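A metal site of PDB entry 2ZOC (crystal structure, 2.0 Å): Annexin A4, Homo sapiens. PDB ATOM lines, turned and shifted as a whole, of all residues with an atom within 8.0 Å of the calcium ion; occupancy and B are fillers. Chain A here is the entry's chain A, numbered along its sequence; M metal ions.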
ATOM      1  N   LEU A 178     -16.459  -0.619  18.340  1.00  0.00           N
ATOM      2  CA  LEU A 178     -15.659   0.358  19.072  1.00  0.00           C
ATOM      3  C   LEU A 178     -16.241   0.582  20.469  1.00  0.00           C
ATOM      4  O   LEU A 178     -15.509   0.817  21.432  1.00  0.00           O
ATOM      5  CB  LEU A 178     -15.608   1.694  18.327  1.00  0.00           C
ATOM      6  CG  LEU A 178     -14.842   1.774  16.982  1.00  0.00           C
ATOM      7  CD1 LEU A 178     -14.985   3.173  16.398  1.00  0.00           C
ATOM      8  CD2 LEU A 178     -13.376   1.428  17.193  1.00  0.00           C
ATOM      9  N   TYR A 179     -17.558   0.493  20.579  1.00  0.00           N
ATOM     10  CA  TYR A 179     -18.244   0.687  21.856  1.00  0.00           C
ATOM     11  C   TYR A 179     -17.991  -0.502  22.778  1.00  0.00           C
ATOM     12  O   TYR A 179     -17.731  -0.332  23.967  1.00  0.00           O
ATOM     13  CB  TYR A 179     -19.752   0.878  21.595  1.00  0.00           C
ATOM     14  CG  TYR A 179     -20.567   1.332  22.792  1.00  0.00           C
ATOM     15  CD1 TYR A 179     -20.046   2.235  23.724  1.00  0.00           C
ATOM     16  CD2 TYR A 179     -21.879   0.897  22.967  1.00  0.00           C
ATOM     17  CE1 TYR A 179     -20.818   2.705  24.792  1.00  0.00           C
ATOM     18  CE2 TYR A 179     -22.652   1.359  24.023  1.00  0.00           C
ATOM     19  CZ  TYR A 179     -22.123   2.255  24.933  1.00  0.00           C
ATOM     20  OH  TYR A 179     -22.894   2.695  25.979  1.00  0.00           O
ATOM     21  N   GLU A 180     -18.068  -1.705  22.206  1.00  0.00           N
ATOM     22  CA  GLU A 180     -17.835  -2.935  22.965  1.00  0.00           C
ATOM     23  C   GLU A 180     -16.367  -3.036  23.392  1.00  0.00           C
ATOM     24  O   GLU A 180     -16.067  -3.516  24.489  1.00  0.00           O
ATOM     25  CB  GLU A 180     -18.179  -4.165  22.115  1.00  0.00           C
ATOM     26  CG  GLU A 180     -19.636  -4.262  21.659  1.00  0.00           C
ATOM     27  CD  GLU A 180     -20.555  -4.830  22.726  1.00  0.00           C
ATOM     28  OE1 GLU A 180     -21.761  -5.015  22.440  1.00  0.00           O
ATOM     29  OE2 GLU A 180     -20.072  -5.105  23.850  1.00  0.00           O
ATOM     30  N   ALA A 181     -15.467  -2.590  22.515  1.00  0.00           N
ATOM     31  CA  ALA A 181     -14.031  -2.669  22.768  1.00  0.00           C
ATOM     32  C   ALA A 181     -13.485  -1.604  23.718  1.00  0.00           C
ATOM     33  O   ALA A 181     -12.342  -1.674  24.154  1.00  0.00           O
ATOM     34  CB  ALA A 181     -13.280  -2.607  21.446  1.00  0.00           C
ATOM     35  N   GLY A 182     -14.300  -0.601  24.046  1.00  0.00           N
ATOM     36  CA  GLY A 182     -13.825   0.440  24.931  1.00  0.00           C
ATOM     37  C   GLY A 182     -14.677   0.681  26.158  1.00  0.00           C
ATOM     38  O   GLY A 182     -14.462   0.079  27.211  1.00  0.00           O
ATOM     39  N   GLU A 183     -15.655   1.566  26.003  1.00  0.00           N
ATOM     40  CA  GLU A 183     -16.565   1.942  27.089  1.00  0.00           C
ATOM     41  C   GLU A 183     -17.160   0.772  27.883  1.00  0.00           C
ATOM     42  O   GLU A 183     -17.130   0.788  29.124  1.00  0.00           O
ATOM     43  CB  GLU A 183     -17.692   2.799  26.523  1.00  0.00           C
ATOM     44  CG  GLU A 183     -18.035   4.034  27.351  1.00  0.00           C
ATOM     45  CD  GLU A 183     -16.856   4.988  27.514  1.00  0.00           C
ATOM     46  OE1 GLU A 183     -16.450   5.660  26.532  1.00  0.00           O
ATOM     47  OE2 GLU A 183     -16.325   5.064  28.638  1.00  0.00           O
ATOM     48  N   LYS A 184     -17.684  -0.231  27.194  1.00  0.00           N
ATOM     49  CA  LYS A 184     -18.308  -1.375  27.856  1.00  0.00           C
ATOM     50  C   LYS A 184     -17.328  -2.475  28.260  1.00  0.00           C
ATOM     51  O   LYS A 184     -17.728  -3.486  28.824  1.00  0.00           O
ATOM     52  CB  LYS A 184     -19.386  -1.977  26.954  1.00  0.00           C
ATOM     53  CG  LYS A 184     -20.370  -0.955  26.413  1.00  0.00           C
ATOM     54  CD  LYS A 184     -21.695  -1.583  26.026  1.00  0.00           C
ATOM     55  CE  LYS A 184     -21.554  -2.601  24.910  1.00  0.00           C
ATOM     56  NZ  LYS A 184     -22.840  -3.317  24.683  1.00  0.00           N
ATOM     57  N   LYS A 185     -16.046  -2.262  27.988  1.00  0.00           N
ATOM     58  CA  LYS A 185     -15.040  -3.265  28.327  1.00  0.00           C
ATOM     59  C   LYS A 185     -14.121  -2.806  29.446  1.00  0.00           C
ATOM     60  O   LYS A 185     -13.832  -1.617  29.571  1.00  0.00           O
ATOM     61  CB  LYS A 185     -14.203  -3.570  27.078  1.00  0.00           C
ATOM     62  CG  LYS A 185     -13.060  -4.552  27.303  1.00  0.00           C
ATOM     63  CD  LYS A 185     -12.172  -4.630  26.066  1.00  0.00           C
ATOM     64  CE  LYS A 185     -11.018  -5.620  26.251  1.00  0.00           C
ATOM     65  NZ  LYS A 185     -11.512  -7.020  26.387  1.00  0.00           N
ATOM     66  N   TRP A 186     -13.676  -3.752  30.278  1.00  0.00           N
ATOM     67  CA  TRP A 186     -12.726  -3.409  31.313  1.00  0.00           C
ATOM     68  C   TRP A 186     -11.452  -3.365  30.496  1.00  0.00           C
ATOM     69  O   TRP A 186     -11.081  -4.350  29.869  1.00  0.00           O
ATOM     70  CB  TRP A 186     -12.628  -4.504  32.388  1.00  0.00           C
ATOM     71  CG  TRP A 186     -11.556  -4.230  33.422  1.00  0.00           C
ATOM     72  CD1 TRP A 186     -10.246  -4.625  33.363  1.00  0.00           C
ATOM     73  CD2 TRP A 186     -11.690  -3.454  34.620  1.00  0.00           C
ATOM     74  NE1 TRP A 186      -9.558  -4.135  34.449  1.00  0.00           N
ATOM     75  CE2 TRP A 186     -10.420  -3.410  35.228  1.00  0.00           C
ATOM     76  CE3 TRP A 186     -12.759  -2.783  35.233  1.00  0.00           C
ATOM     77  CZ2 TRP A 186     -10.183  -2.731  36.436  1.00  0.00           C
ATOM     78  CZ3 TRP A 186     -12.526  -2.099  36.429  1.00  0.00           C
ATOM     79  CH2 TRP A 186     -11.244  -2.076  37.015  1.00  0.00           C
ATOM     80  N   GLY A 187     -10.786  -2.211  30.478  1.00  0.00           N
ATOM     81  CA  GLY A 187      -9.593  -2.107  29.667  1.00  0.00           C
ATOM     82  C   GLY A 187     -10.042  -1.750  28.258  1.00  0.00           C
ATOM     83  O   GLY A 187     -11.128  -1.205  28.072  1.00  0.00           O
ATOM     84  N   THR A 188      -9.226  -2.078  27.258  1.00  0.00           N
ATOM     85  CA  THR A 188      -9.555  -1.723  25.885  1.00  0.00           C
ATOM     86  C   THR A 188      -8.992  -2.694  24.853  1.00  0.00           C
ATOM     87  O   THR A 188      -7.870  -3.174  25.005  1.00  0.00           O
ATOM     88  CB  THR A 188      -8.965  -0.335  25.539  1.00  0.00           C
ATOM     89  OG1 THR A 188      -9.260   0.578  26.602  1.00  0.00           O
ATOM     90  CG2 THR A 188      -9.568   0.187  24.238  1.00  0.00           C
ATOM     91  N   ASP A 189      -9.769  -2.990  23.824  1.00  0.00           N
ATOM     92  CA  ASP A 189      -9.265  -3.842  22.751  1.00  0.00           C
ATOM     93  C   ASP A 189      -8.721  -2.762  21.816  1.00  0.00           C
ATOM     94  O   ASP A 189      -9.403  -2.304  20.906  1.00  0.00           O
ATOM     95  CB  ASP A 189     -10.386  -4.615  22.068  1.00  0.00           C
ATOM     96  CG  ASP A 189      -9.856  -5.644  21.065  1.00  0.00           C
ATOM     97  OD1 ASP A 189      -8.860  -5.334  20.379  1.00  0.00           O
ATOM     98  OD2 ASP A 189     -10.446  -6.736  20.960  1.00  0.00           O
ATOM     99  N   PHE A 193      -9.677  -0.548  17.802  1.00  0.00           N
ATOM    100  CA  PHE A 193      -9.696   0.888  17.545  1.00  0.00           C
ATOM    101  C   PHE A 193      -8.778   1.235  16.378  1.00  0.00           C
ATOM    102  O   PHE A 193      -9.214   1.842  15.400  1.00  0.00           O
ATOM    103  CB  PHE A 193      -9.221   1.669  18.774  1.00  0.00           C
ATOM    104  CG  PHE A 193     -10.307   1.947  19.770  1.00  0.00           C
ATOM    105  CD1 PHE A 193     -10.773   0.955  20.616  1.00  0.00           C
ATOM    106  CD2 PHE A 193     -10.887   3.221  19.843  1.00  0.00           C
ATOM    107  CE1 PHE A 193     -11.789   1.216  21.539  1.00  0.00           C
ATOM    108  CE2 PHE A 193     -11.900   3.490  20.760  1.00  0.00           C
ATOM    109  CZ  PHE A 193     -12.353   2.494  21.608  1.00  0.00           C
ATOM    110  N   SER A 223     -14.063   9.032  24.163  1.00  0.00           N
ATOM    111  CA  SER A 223     -13.787   7.645  24.534  1.00  0.00           C
ATOM    112  C   SER A 223     -12.313   7.314  24.344  1.00  0.00           C
ATOM    113  O   SER A 223     -11.717   6.637  25.186  1.00  0.00           O
ATOM    114  CB  SER A 223     -14.657   6.693  23.700  1.00  0.00           C
ATOM    115  OG  SER A 223     -16.004   6.732  24.151  1.00  0.00           O
ATOM    116  N   SER A 226     -10.481   8.745  27.260  1.00  0.00           N
ATOM    117  CA  SER A 226     -10.720   8.022  28.507  1.00  0.00           C
ATOM    118  C   SER A 226     -10.265   6.562  28.459  1.00  0.00           C
ATOM    119  O   SER A 226      -9.952   5.963  29.493  1.00  0.00           O
ATOM    120  CB  SER A 226     -12.206   8.093  28.900  1.00  0.00           C
ATOM    121  OG  SER A 226     -13.048   7.428  27.974  1.00  0.00           O
ATOM    122  N   GLU A 227     -10.188   5.990  27.262  1.00  0.00           N
ATOM    123  CA  GLU A 227      -9.766   4.587  27.120  1.00  0.00           C
ATOM    124  C   GLU A 227      -8.272   4.369  26.898  1.00  0.00           C
ATOM    125  O   GLU A 227      -7.720   3.362  27.327  1.00  0.00           O
ATOM    126  CB  GLU A 227     -10.543   3.930  25.980  1.00  0.00           C
ATOM    127  CG  GLU A 227     -12.014   3.733  26.271  1.00  0.00           C
ATOM    128  CD  GLU A 227     -12.259   2.605  27.247  1.00  0.00           C
ATOM    129  OE1 GLU A 227     -13.239   2.690  28.043  1.00  0.00           O
ATOM    130  OE2 GLU A 227     -11.492   1.612  27.216  1.00  0.00           O
ATOM    131  N   THR A 228      -7.613   5.310  26.227  1.00  0.00           N
ATOM    132  CA  THR A 228      -6.187   5.172  25.941  1.00  0.00           C
ATOM    133  C   THR A 228      -5.329   6.267  26.581  1.00  0.00           C
ATOM    134  O   THR A 228      -5.848   7.156  27.254  1.00  0.00           O
ATOM    135  CB  THR A 228      -5.930   5.196  24.427  1.00  0.00           C
ATOM    136  OG1 THR A 228      -6.375   6.444  23.882  1.00  0.00           O
ATOM    137  CG2 THR A 228      -6.672   4.041  23.745  1.00  0.00           C
HETATM  138 CA    CA M   1     -12.858   0.282  28.620  1.00  0.00          CA
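OE1 of Glu 227 sits close to N of Glu 183 (3.4 Å).
O of Glu 227 sits at hydrogen-bond distance from OG1 of Thr 188 (3.3 Å).
Within 4 Å of the calcium ion: Gly 182, Lys 185, Gly 187 and Glu 227.
The calcium ion is bound by O of Gly 182, at 2.1 Å.
The calcium ion is bound by the backbone carbonyl oxygen (O) of Lys 185 (2.3 Å).
O of Gly 187 binds the calcium ion, 2.3 Å away.
The calcium ion is bound by OE2 of Glu 227 (2.4 Å).
OE1 of Glu 227 binds the calcium ion.
The calcium ion has five donor atoms within binding distance.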
